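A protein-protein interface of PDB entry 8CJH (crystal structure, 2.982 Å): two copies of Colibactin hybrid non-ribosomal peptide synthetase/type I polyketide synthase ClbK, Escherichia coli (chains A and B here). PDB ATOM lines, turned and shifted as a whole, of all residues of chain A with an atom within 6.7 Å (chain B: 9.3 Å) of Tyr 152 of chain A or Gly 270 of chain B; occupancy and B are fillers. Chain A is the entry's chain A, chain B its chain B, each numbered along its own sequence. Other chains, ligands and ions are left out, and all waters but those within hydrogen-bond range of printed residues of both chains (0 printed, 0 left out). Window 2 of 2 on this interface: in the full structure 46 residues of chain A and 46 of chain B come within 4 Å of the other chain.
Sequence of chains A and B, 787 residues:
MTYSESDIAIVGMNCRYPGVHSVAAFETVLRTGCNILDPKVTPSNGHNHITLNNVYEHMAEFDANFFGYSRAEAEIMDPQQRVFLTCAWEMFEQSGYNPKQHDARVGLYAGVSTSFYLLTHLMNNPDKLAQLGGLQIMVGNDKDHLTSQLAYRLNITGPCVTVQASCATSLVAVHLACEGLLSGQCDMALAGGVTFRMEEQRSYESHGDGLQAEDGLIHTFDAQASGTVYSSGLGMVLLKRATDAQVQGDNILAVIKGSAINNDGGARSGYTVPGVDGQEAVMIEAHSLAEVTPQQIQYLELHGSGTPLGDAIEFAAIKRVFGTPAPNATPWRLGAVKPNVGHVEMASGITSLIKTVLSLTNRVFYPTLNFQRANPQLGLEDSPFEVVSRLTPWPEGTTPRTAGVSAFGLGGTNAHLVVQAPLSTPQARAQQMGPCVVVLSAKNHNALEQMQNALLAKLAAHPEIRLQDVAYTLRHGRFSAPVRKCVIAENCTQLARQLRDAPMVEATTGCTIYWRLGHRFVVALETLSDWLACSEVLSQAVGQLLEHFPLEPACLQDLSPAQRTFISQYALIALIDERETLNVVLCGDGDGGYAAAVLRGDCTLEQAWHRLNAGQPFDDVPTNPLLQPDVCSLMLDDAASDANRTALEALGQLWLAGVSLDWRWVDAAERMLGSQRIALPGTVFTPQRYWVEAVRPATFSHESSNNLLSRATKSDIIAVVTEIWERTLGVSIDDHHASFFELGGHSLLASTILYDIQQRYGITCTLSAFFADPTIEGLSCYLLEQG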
ATOM      1  N   PHE A  67     -38.481   4.963  15.828  1.00  0.00           N
ATOM      2  CA  PHE A  67     -37.213   5.303  15.207  1.00  0.00           C
ATOM      3  C   PHE A  67     -37.408   6.098  13.922  1.00  0.00           C
ATOM      4  O   PHE A  67     -36.440   6.418  13.249  1.00  0.00           O
ATOM      5  CB  PHE A  67     -36.418   4.032  14.960  1.00  0.00           C
ATOM      6  CG  PHE A  67     -35.857   3.444  16.222  1.00  0.00           C
ATOM      7  CD1 PHE A  67     -34.787   4.046  16.852  1.00  0.00           C
ATOM      8  CD2 PHE A  67     -36.413   2.310  16.789  1.00  0.00           C
ATOM      9  CE1 PHE A  67     -34.258   3.509  18.014  1.00  0.00           C
ATOM     10  CE2 PHE A  67     -35.889   1.775  17.953  1.00  0.00           C
ATOM     11  CZ  PHE A  67     -34.808   2.375  18.562  1.00  0.00           C
ATOM     12  N   GLY A  68     -38.652   6.409  13.580  1.00  0.00           N
ATOM     13  CA  GLY A  68     -38.920   7.327  12.490  1.00  0.00           C
ATOM     14  C   GLY A  68     -38.833   6.661  11.121  1.00  0.00           C
ATOM     15  O   GLY A  68     -38.447   7.299  10.142  1.00  0.00           O
ATOM     16  N   TYR A  69     -39.203   5.378  11.064  1.00  0.00           N
ATOM     17  CA  TYR A  69     -39.204   4.633   9.819  1.00  0.00           C
ATOM     18  C   TYR A  69     -40.623   4.522   9.298  1.00  0.00           C
ATOM     19  O   TYR A  69     -41.537   4.305  10.078  1.00  0.00           O
ATOM     20  CB  TYR A  69     -38.639   3.229  10.029  1.00  0.00           C
ATOM     21  CG  TYR A  69     -37.142   3.159  10.091  1.00  0.00           C
ATOM     22  CD1 TYR A  69     -36.389   3.235   8.935  1.00  0.00           C
ATOM     23  CD2 TYR A  69     -36.484   3.032  11.298  1.00  0.00           C
ATOM     24  CE1 TYR A  69     -35.009   3.163   8.970  1.00  0.00           C
ATOM     25  CE2 TYR A  69     -35.107   2.969  11.357  1.00  0.00           C
ATOM     26  CZ  TYR A  69     -34.365   3.032  10.189  1.00  0.00           C
ATOM     27  OH  TYR A  69     -32.990   2.973  10.241  1.00  0.00           O
ATOM     28  N   LYS A 100     -29.635   9.659  22.068  1.00  0.00           N
ATOM     29  CA  LYS A 100     -29.652  10.563  20.931  1.00  0.00           C
ATOM     30  C   LYS A 100     -28.822  11.818  21.223  1.00  0.00           C
ATOM     31  O   LYS A 100     -28.663  12.654  20.340  1.00  0.00           O
ATOM     32  CB  LYS A 100     -31.097  10.873  20.491  1.00  0.00           C
ATOM     33  CG  LYS A 100     -31.200  11.453  19.078  1.00  0.00           C
ATOM     34  CD  LYS A 100     -32.544  11.986  18.626  1.00  0.00           C
ATOM     35  CE  LYS A 100     -32.376  12.928  17.443  1.00  0.00           C
ATOM     36  NZ  LYS A 100     -33.670  13.453  16.948  1.00  0.00           N
ATOM     37  N   LEU A 108     -18.791   4.150  16.288  1.00  0.00           N
ATOM     38  CA  LEU A 108     -19.555   2.962  15.963  1.00  0.00           C
ATOM     39  C   LEU A 108     -18.680   2.022  15.156  1.00  0.00           C
ATOM     40  O   LEU A 108     -18.255   2.336  14.037  1.00  0.00           O
ATOM     41  CB  LEU A 108     -20.790   3.370  15.169  1.00  0.00           C
ATOM     42  CG  LEU A 108     -21.856   4.066  15.992  1.00  0.00           C
ATOM     43  CD1 LEU A 108     -22.940   4.607  15.092  1.00  0.00           C
ATOM     44  CD2 LEU A 108     -22.433   3.098  17.007  1.00  0.00           C
ATOM     45  N   THR A 147     -23.878   0.563  10.563  1.00  0.00           N
ATOM     46  CA  THR A 147     -23.394   1.630  11.421  1.00  0.00           C
ATOM     47  C   THR A 147     -24.089   2.940  11.065  1.00  0.00           C
ATOM     48  O   THR A 147     -24.613   3.597  11.957  1.00  0.00           O
ATOM     49  CB  THR A 147     -21.870   1.740  11.373  1.00  0.00           C
ATOM     50  OG1 THR A 147     -21.471   1.950  10.017  1.00  0.00           O
ATOM     51  CG2 THR A 147     -21.192   0.511  11.946  1.00  0.00           C
ATOM     52  N   SER A 148     -24.144   3.283   9.766  1.00  0.00           N
ATOM     53  CA  SER A 148     -24.628   4.586   9.313  1.00  0.00           C
ATOM     54  C   SER A 148     -26.010   4.876   9.888  1.00  0.00           C
ATOM     55  O   SER A 148     -26.289   5.993  10.308  1.00  0.00           O
ATOM     56  CB  SER A 148     -24.736   4.658   7.797  1.00  0.00           C
ATOM     57  OG  SER A 148     -23.660   4.021   7.139  1.00  0.00           O
ATOM     58  N   GLN A 149     -26.882   3.861   9.855  1.00  0.00           N
ATOM     59  CA  GLN A 149     -28.212   3.943  10.432  1.00  0.00           C
ATOM     60  C   GLN A 149     -28.094   4.320  11.899  1.00  0.00           C
ATOM     61  O   GLN A 149     -28.631   5.337  12.322  1.00  0.00           O
ATOM     62  CB  GLN A 149     -28.956   2.619  10.260  1.00  0.00           C
ATOM     63  CG  GLN A 149     -29.549   2.412   8.871  1.00  0.00           C
ATOM     64  CD  GLN A 149     -30.694   3.356   8.596  1.00  0.00           C
ATOM     65  OE1 GLN A 149     -31.000   4.243   9.395  1.00  0.00           O
ATOM     66  NE2 GLN A 149     -31.338   3.175   7.454  1.00  0.00           N
ATOM     67  N   LEU A 150     -27.356   3.517  12.667  1.00  0.00           N
ATOM     68  CA  LEU A 150     -27.227   3.777  14.092  1.00  0.00           C
ATOM     69  C   LEU A 150     -26.726   5.197  14.311  1.00  0.00           C
ATOM     70  O   LEU A 150     -27.192   5.879  15.205  1.00  0.00           O
ATOM     71  CB  LEU A 150     -26.279   2.766  14.739  1.00  0.00           C
ATOM     72  CG  LEU A 150     -26.969   1.553  15.359  1.00  0.00           C
ATOM     73  CD1 LEU A 150     -27.614   0.678  14.292  1.00  0.00           C
ATOM     74  CD2 LEU A 150     -25.986   0.741  16.184  1.00  0.00           C
ATOM     75  N   ALA A 151     -25.778   5.627  13.483  1.00  0.00           N
ATOM     76  CA  ALA A 151     -25.188   6.947  13.607  1.00  0.00           C
ATOM     77  C   ALA A 151     -26.255   8.006  13.392  1.00  0.00           C
ATOM     78  O   ALA A 151     -26.236   9.050  14.026  1.00  0.00           O
ATOM     79  CB  ALA A 151     -24.061   7.112  12.616  1.00  0.00           C
ATOM     80  N   TYR A 152     -27.182   7.734  12.479  1.00  0.00           N
ATOM     81  CA  TYR A 152     -28.280   8.651  12.258  1.00  0.00           C
ATOM     82  C   TYR A 152     -29.165   8.639  13.490  1.00  0.00           C
ATOM     83  O   TYR A 152     -29.287   9.645  14.166  1.00  0.00           O
ATOM     84  CB  TYR A 152     -29.064   8.264  11.009  1.00  0.00           C
ATOM     85  CG  TYR A 152     -30.224   9.166  10.694  1.00  0.00           C
ATOM     86  CD1 TYR A 152     -30.092  10.543  10.718  1.00  0.00           C
ATOM     87  CD2 TYR A 152     -31.451   8.637  10.335  1.00  0.00           C
ATOM     88  CE1 TYR A 152     -31.157  11.368  10.411  1.00  0.00           C
ATOM     89  CE2 TYR A 152     -32.525   9.451  10.019  1.00  0.00           C
ATOM     90  CZ  TYR A 152     -32.380  10.822  10.057  1.00  0.00           C
ATOM     91  OH  TYR A 152     -33.460  11.614   9.735  1.00  0.00           O
ATOM     92  N   ARG A 153     -29.711   7.466  13.801  1.00  0.00           N
ATOM     93  CA  ARG A 153     -30.784   7.351  14.773  1.00  0.00           C
ATOM     94  C   ARG A 153     -30.328   7.728  16.183  1.00  0.00           C
ATOM     95  O   ARG A 153     -31.132   8.225  16.967  1.00  0.00           O
ATOM     96  CB  ARG A 153     -31.346   5.934  14.779  1.00  0.00           C
ATOM     97  CG  ARG A 153     -31.778   5.424  13.411  1.00  0.00           C
ATOM     98  CD  ARG A 153     -32.943   6.156  12.791  1.00  0.00           C
ATOM     99  NE  ARG A 153     -33.043   5.814  11.379  1.00  0.00           N
ATOM    100  CZ  ARG A 153     -34.007   6.223  10.570  1.00  0.00           C
ATOM    101  NH1 ARG A 153     -35.040   6.889  11.046  1.00  0.00           N
ATOM    102  NH2 ARG A 153     -33.949   5.942   9.282  1.00  0.00           N
ATOM    103  N   LEU A 154     -29.055   7.494  16.516  1.00  0.00           N
ATOM    104  CA  LEU A 154     -28.534   7.870  17.825  1.00  0.00           C
ATOM    105  C   LEU A 154     -27.721   9.156  17.706  1.00  0.00           C
ATOM    106  O   LEU A 154     -26.983   9.516  18.620  1.00  0.00           O
ATOM    107  CB  LEU A 154     -27.659   6.751  18.388  1.00  0.00           C
ATOM    108  CG  LEU A 154     -28.251   5.341  18.364  1.00  0.00           C
ATOM    109  CD1 LEU A 154     -27.630   4.471  19.439  1.00  0.00           C
ATOM    110  CD2 LEU A 154     -29.743   5.347  18.536  1.00  0.00           C
ATOM    111  N   ASN A 155     -27.850   9.841  16.568  1.00  0.00           N
ATOM    112  CA  ASN A 155     -27.217  11.130  16.399  1.00  0.00           C
ATOM    113  C   ASN A 155     -25.776  11.073  16.890  1.00  0.00           C
ATOM    114  O   ASN A 155     -25.405  11.834  17.782  1.00  0.00           O
ATOM    115  CB  ASN A 155     -27.959  12.207  17.170  1.00  0.00           C
ATOM    116  CG  ASN A 155     -27.386  13.575  16.933  1.00  0.00           C
ATOM    117  OD1 ASN A 155     -26.510  13.774  16.101  1.00  0.00           O
ATOM    118  ND2 ASN A 155     -27.918  14.540  17.642  1.00  0.00           N
ATOM    119  N   ILE A 156     -25.013  10.148  16.289  1.00  0.00           N
ATOM    120  CA  ILE A 156     -23.616   9.916  16.581  1.00  0.00           C
ATOM    121  C   ILE A 156     -22.789  10.473  15.439  1.00  0.00           C
ATOM    122  O   ILE A 156     -23.067  10.168  14.289  1.00  0.00           O
ATOM    123  CB  ILE A 156     -23.371   8.415  16.760  1.00  0.00           C
ATOM    124  CG1 ILE A 156     -24.086   7.895  18.005  1.00  0.00           C
ATOM    125  CG2 ILE A 156     -21.886   8.110  16.793  1.00  0.00           C
ATOM    126  CD1 ILE A 156     -24.067   6.388  18.134  1.00  0.00           C
ATOM    127  N   CYS A 160     -17.488   6.102  12.229  1.00  0.00           N
ATOM    128  CA  CYS A 160     -18.618   5.243  11.985  1.00  0.00           C
ATOM    129  C   CYS A 160     -18.212   4.254  10.905  1.00  0.00           C
ATOM    130  O   CYS A 160     -18.074   4.628   9.741  1.00  0.00           O
ATOM    131  CB  CYS A 160     -19.813   6.098  11.605  1.00  0.00           C
ATOM    132  SG  CYS A 160     -21.337   5.145  11.462  1.00  0.00           S
ATOM    133  N   ASN B 263     -19.475  10.852  11.013  1.00  0.00           N
ATOM    134  CA  ASN B 263     -20.813  10.710  10.479  1.00  0.00           C
ATOM    135  C   ASN B 263     -21.606  11.994  10.721  1.00  0.00           C
ATOM    136  O   ASN B 263     -21.367  12.699  11.693  1.00  0.00           O
ATOM    137  CB  ASN B 263     -21.505   9.479  11.060  1.00  0.00           C
ATOM    138  CG  ASN B 263     -22.818   9.185  10.367  1.00  0.00           C
ATOM    139  OD1 ASN B 263     -23.829   9.814  10.679  1.00  0.00           O
ATOM    140  ND2 ASN B 263     -22.809   8.241   9.434  1.00  0.00           N
ATOM    141  N   ASP B 264     -22.549  12.281   9.813  1.00  0.00           N
ATOM    142  CA  ASP B 264     -23.381  13.476   9.866  1.00  0.00           C
ATOM    143  C   ASP B 264     -24.294  13.426  11.082  1.00  0.00           C
ATOM    144  O   ASP B 264     -24.980  14.406  11.402  1.00  0.00           O
ATOM    145  CB  ASP B 264     -24.242  13.605   8.608  1.00  0.00           C
ATOM    146  CG  ASP B 264     -23.470  13.856   7.328  1.00  0.00           C
ATOM    147  OD1 ASP B 264     -22.330  14.347   7.419  1.00  0.00           O
ATOM    148  OD2 ASP B 264     -24.015  13.544   6.245  1.00  0.00           O
ATOM    149  N   GLY B 265     -24.305  12.256  11.729  1.00  0.00           N
ATOM    150  CA  GLY B 265     -25.142  12.035  12.888  1.00  0.00           C
ATOM    151  C   GLY B 265     -26.598  12.308  12.553  1.00  0.00           C
ATOM    152  O   GLY B 265     -27.064  11.969  11.470  1.00  0.00           O
ATOM    153  N   GLY B 266     -27.282  12.953  13.496  1.00  0.00           N
ATOM    154  CA  GLY B 266     -28.677  13.307  13.342  1.00  0.00           C
ATOM    155  C   GLY B 266     -28.859  14.709  12.778  1.00  0.00           C
ATOM    156  O   GLY B 266     -29.966  15.204  12.776  1.00  0.00           O
ATOM    157  N   ALA B 267     -27.787  15.330  12.272  1.00  0.00           N
ATOM    158  CA  ALA B 267     -27.870  16.710  11.807  1.00  0.00           C
ATOM    159  C   ALA B 267     -28.187  16.750  10.318  1.00  0.00           C
ATOM    160  O   ALA B 267     -27.409  17.301   9.542  1.00  0.00           O
ATOM    161  CB  ALA B 267     -26.570  17.427  12.092  1.00  0.00           C
ATOM    162  N   ARG B 268     -29.332  16.169   9.944  1.00  0.00           N
ATOM    163  CA  ARG B 268     -29.727  16.056   8.551  1.00  0.00           C
ATOM    164  C   ARG B 268     -31.234  15.851   8.451  1.00  0.00           C
ATOM    165  O   ARG B 268     -31.859  15.371   9.387  1.00  0.00           O
ATOM    166  CB  ARG B 268     -29.017  14.869   7.911  1.00  0.00           C
ATOM    167  CG  ARG B 268     -29.499  13.528   8.447  1.00  0.00           C
ATOM    168  CD  ARG B 268     -28.829  12.301   7.839  1.00  0.00           C
ATOM    169  NE  ARG B 268     -27.694  11.846   8.613  1.00  0.00           N
ATOM    170  CZ  ARG B 268     -27.174  10.639   8.528  1.00  0.00           C
ATOM    171  NH1 ARG B 268     -27.635   9.768   7.648  1.00  0.00           N
ATOM    172  NH2 ARG B 268     -26.182  10.306   9.331  1.00  0.00           N
ATOM    173  N   SER B 269     -31.808  16.174   7.289  1.00  0.00           N
ATOM    174  CA  SER B 269     -33.256  16.169   7.119  1.00  0.00           C
ATOM    175  C   SER B 269     -33.813  14.760   6.912  1.00  0.00           C
ATOM    176  O   SER B 269     -35.012  14.587   6.772  1.00  0.00           O
ATOM    177  CB  SER B 269     -33.639  17.059   5.972  1.00  0.00           C
ATOM    178  OG  SER B 269     -33.030  16.622   4.769  1.00  0.00           O
ATOM    179  N   GLY B 270     -32.954  13.747   6.872  1.00  0.00           N
ATOM    180  CA  GLY B 270     -33.400  12.385   6.626  1.00  0.00           C
ATOM    181  C   GLY B 270     -32.221  11.489   6.277  1.00  0.00           C
ATOM    182  O   GLY B 270     -31.210  11.971   5.782  1.00  0.00           O
ATOM    183  N   TYR B 271     -32.361  10.189   6.513  1.00  0.00           N
ATOM    184  CA  TYR B 271     -31.215   9.297   6.488  1.00  0.00           C
ATOM    185  C   TYR B 271     -30.294   9.571   5.301  1.00  0.00           C
ATOM    186  O   TYR B 271     -29.071   9.616   5.464  1.00  0.00           O
ATOM    187  CB  TYR B 271     -31.634   7.828   6.442  1.00  0.00           C
ATOM    188  CG  TYR B 271     -30.456   6.895   6.384  1.00  0.00           C
ATOM    189  CD1 TYR B 271     -29.647   6.712   7.480  1.00  0.00           C
ATOM    190  CD2 TYR B 271     -30.102   6.251   5.218  1.00  0.00           C
ATOM    191  CE1 TYR B 271     -28.542   5.874   7.438  1.00  0.00           C
ATOM    192  CE2 TYR B 271     -29.004   5.410   5.157  1.00  0.00           C
ATOM    193  CZ  TYR B 271     -28.222   5.212   6.272  1.00  0.00           C
ATOM    194  OH  TYR B 271     -27.137   4.384   6.217  1.00  0.00           O
ATOM    195  N   THR B 272     -30.882   9.743   4.109  1.00  0.00           N
ATOM    196  CA  THR B 272     -30.110   9.738   2.878  1.00  0.00           C
ATOM    197  C   THR B 272     -29.705  11.146   2.475  1.00  0.00           C
ATOM    198  O   THR B 272     -29.416  11.387   1.313  1.00  0.00           O
ATOM    199  CB  THR B 272     -30.913   9.152   1.715  1.00  0.00           C
ATOM    200  OG1 THR B 272     -31.884  10.137   1.372  1.00  0.00           O
ATOM    201  CG2 THR B 272     -31.581   7.838   2.043  1.00  0.00           C
ATOM    202  N   VAL B 273     -29.696  12.072   3.425  1.00  0.00           N
ATOM    203  CA  VAL B 273     -29.381  13.452   3.118  1.00  0.00           C
ATOM    204  C   VAL B 273     -28.040  13.819   3.740  1.00  0.00           C
ATOM    205  O   VAL B 273     -27.731  13.459   4.872  1.00  0.00           O
ATOM    206  CB  VAL B 273     -30.492  14.394   3.602  1.00  0.00           C
ATOM    207  CG1 VAL B 273     -30.198  15.831   3.228  1.00  0.00           C
ATOM    208  CG2 VAL B 273     -31.842  13.970   3.060  1.00  0.00           C
ATOM    209  N   PRO B 274     -27.192  14.548   3.000  1.00  0.00           N
ATOM    210  CA  PRO B 274     -25.962  15.103   3.561  1.00  0.00           C
ATOM    211  C   PRO B 274     -26.189  16.103   4.693  1.00  0.00           C
ATOM    212  O   PRO B 274     -27.218  16.776   4.734  1.00  0.00           O
ATOM    213  CB  PRO B 274     -25.318  15.802   2.357  1.00  0.00           C
ATOM    214  CG  PRO B 274     -25.925  15.103   1.162  1.00  0.00           C
ATOM    215  CD  PRO B 274     -27.349  14.824   1.569  1.00  0.00           C
ATOM    216  N   GLY B 275     -25.197  16.193   5.592  1.00  0.00           N
ATOM    217  CA  GLY B 275     -25.252  17.036   6.776  1.00  0.00           C
ATOM    218  C   GLY B 275     -24.103  18.040   6.812  1.00  0.00           C
ATOM    219  O   GLY B 275     -22.950  17.688   7.112  1.00  0.00           O
ATOM    220  N   LEU B 309     -28.865  18.918  -4.375  1.00  0.00           N
ATOM    221  CA  LEU B 309     -28.832  19.105  -2.943  1.00  0.00           C
ATOM    222  C   LEU B 309     -27.450  18.755  -2.392  1.00  0.00           C
ATOM    223  O   LEU B 309     -26.878  19.513  -1.598  1.00  0.00           O
ATOM    224  CB  LEU B 309     -29.928  18.222  -2.346  1.00  0.00           C
ATOM    225  CG  LEU B 309     -30.217  18.453  -0.869  1.00  0.00           C
ATOM    226  CD1 LEU B 309     -30.706  19.873  -0.636  1.00  0.00           C
ATOM    227  CD2 LEU B 309     -31.221  17.445  -0.343  1.00  0.00           C
ATOM    228  N   ILE B 313     -25.004  21.317  -0.529  1.00  0.00           N
ATOM    229  CA  ILE B 313     -24.574  21.146   0.849  1.00  0.00           C
ATOM    230  C   ILE B 313     -23.054  21.116   0.920  1.00  0.00           C
ATOM    231  O   ILE B 313     -22.437  21.902   1.651  1.00  0.00           O
ATOM    232  CB  ILE B 313     -25.177  19.868   1.441  1.00  0.00           C
ATOM    233  CG1 ILE B 313     -26.690  20.003   1.594  1.00  0.00           C
ATOM    234  CG2 ILE B 313     -24.496  19.509   2.755  1.00  0.00           C
ATOM    235  CD1 ILE B 313     -27.390  18.696   1.877  1.00  0.00           C
ATOM    236  N   GLY B 409     -20.329   9.619   2.203  1.00  0.00           N
ATOM    237  CA  GLY B 409     -21.118   8.462   1.843  1.00  0.00           C
ATOM    238  C   GLY B 409     -22.585   8.622   2.195  1.00  0.00           C
ATOM    239  O   GLY B 409     -22.934   9.213   3.212  1.00  0.00           O
ATOM    240  N   LEU B 410     -23.431   8.068   1.332  1.00  0.00           N
ATOM    241  CA  LEU B 410     -24.835   7.956   1.638  1.00  0.00           C
ATOM    242  C   LEU B 410     -24.946   7.256   2.985  1.00  0.00           C
ATOM    243  O   LEU B 410     -24.253   6.274   3.232  1.00  0.00           O
ATOM    244  CB  LEU B 410     -25.516   7.188   0.510  1.00  0.00           C
ATOM    245  CG  LEU B 410     -27.027   7.028   0.635  1.00  0.00           C
ATOM    246  CD1 LEU B 410     -27.666   6.786  -0.720  1.00  0.00           C
ATOM    247  CD2 LEU B 410     -27.369   5.875   1.553  1.00  0.00           C
ATOM    248  N   GLY B 411     -25.798   7.801   3.859  1.00  0.00           N
ATOM    249  CA  GLY B 411     -25.911   7.314   5.218  1.00  0.00           C
ATOM    250  C   GLY B 411     -25.125   8.195   6.181  1.00  0.00           C
ATOM    251  O   GLY B 411     -25.196   8.007   7.393  1.00  0.00           O
ATOM    252  N   GLY B 412     -24.366   9.141   5.614  1.00  0.00           N
ATOM    253  CA  GLY B 412     -23.757  10.212   6.378  1.00  0.00           C
ATOM    254  C   GLY B 412     -22.362   9.888   6.905  1.00  0.00           C
ATOM    255  O   GLY B 412     -21.794  10.684   7.642  1.00  0.00           O
ATOM    256  N   THR B 413     -21.802   8.730   6.538  1.00  0.00           N
ATOM    257  CA  THR B 413     -20.439   8.428   6.937  1.00  0.00           C
ATOM    258  C   THR B 413     -19.486   9.173   6.009  1.00  0.00           C
ATOM    259  O   THR B 413     -19.528   8.957   4.805  1.00  0.00           O
ATOM    260  CB  THR B 413     -20.141   6.929   6.906  1.00  0.00           C
ATOM    261  OG1 THR B 413     -21.116   6.254   7.687  1.00  0.00           O
ATOM    262  CG2 THR B 413     -18.791   6.599   7.494  1.00  0.00           C
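Hydrophobic or aromatic side chains of chain A within 4 Å of the printed part of chain B: Ala 151 and Tyr 152.
Among the printed residues, pairs that only touch across the chains: Ser 148 of chain A with Tyr 271 of chain B (2.9 Å), Ser 148 of chain A with Gly 411 of chain B (3.4 Å), Gln 149 of chain A with Tyr 271 of chain B (3.4 Å), Ala 151 of chain A with Asn 263 of chain B (3.3 Å), Ala 151 of chain A with Gly 265 of chain B (3.4 Å), Tyr 152 of chain A with Gly 265 of chain B (3.4 Å), Tyr 152 of chain A with Gly 266 of chain B (3.8 Å), Tyr 152 of chain A with Arg 268 of chain B (3.4 Å), Tyr 152 of chain A with Gly 270 of chain B (3.2 Å), Tyr 152 of chain A with Tyr 271 of chain B (3.6 Å), Asn 155 of chain A with Gly 265 of chain B (3.8 Å), Ile 156 of chain A with Asn 263 of chain B (3.7 Å), Ile 156 of chain A with Gly 265 of chain B (3.1 Å), Cys 160 of chain A with Asn 263 of chain B (3.8 Å) and Cys 160 of chain A with Thr 413 of chain B (3.1 Å).
OE1 of Gln 149 of chain A sits at hydrogen-bond distance from NE of Arg 153 of chain A (3.3 Å).
O of Ala 151 of chain A is in hydrogen-bond range of N of Ile 156 of chain A (2.8 Å).
The side-chain amide oxygen (OD1) of Asn 263 of chain B sits at hydrogen-bond distance from the backbone NH (N) of Gly 265 of chain B, 2.7 Å away.
The side-chain amide oxygen (OD1) of Asn 263 of chain B is in hydrogen-bond range of the guanidinium group (NH2) of Arg 268 of chain B (2.8 Å).
The backbone carbonyl oxygen (O) of Gly 411 of chain B lies within hydrogen-bond range of the side-chain amide nitrogen (ND2) of Asn 263 of chain B, at 3.1 Å.
The side-chain amide nitrogen (ND2) of Asn 263 of chain B sits close to the backbone NH (N) of Thr 413 of chain B (3.1 Å).
Tyr 152 of chain A touches just these residues of chain B: Gly 265 (3.4 Å), Gly 266 (3.8 Å), Arg 268 (3.4 Å), Gly 270 (3.2 Å) and Tyr 271 (3.6 Å).
Of chain A, only Tyr 152 comes within 4 Å of Gly 270 of chain B.
Ala 151 of chain A touches just these residues of chain B: Asn 263 and Gly 265.
No residue of chain B comes within 4 Å of Arg 153 of chain A.
Of the printed residues of chain A, Thr 413 of chain B touches Ser 148 and Cys 160.
Printed residues of chain B within 4 Å of Ile 156 of chain A: Asn 263 (3.7 Å) and Gly 265 (3.1 Å).
Of the printed residues of chain A, Gly 265 of chain B touches Ala 151 (3.4 Å), Tyr 152 (3.4 Å), Asn 155 (3.8 Å) and Ile 156 (3.1 Å).
Printed residues of chain A within 4 Å of Asn 263 of chain B: Ala 151, Ile 156 and Cys 160.
Gly 412 of chain B touches none of the printed residues of chain A.
The nearest residue of chain A that does not touch Gly 270 of chain B is Arg 153 of chain A (6.5 Å).
The nearest printed residue of chain A that does not touch Gly 411 of chain B is Gln 149 of chain A (5.1 Å).
No position is printed for both chains.
The side-chain hydroxyl (OG) of Ser 148 of chain A is in hydrogen-bond range of the side-chain hydroxyl (OG1) of Thr 413 of chain B, 3.4 Å away.
The side-chain amide oxygen (OD1) of Asn 155 of chain A lies within hydrogen-bond range of the backbone NH (N) of Gly 266 of chain B (2.8 Å).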
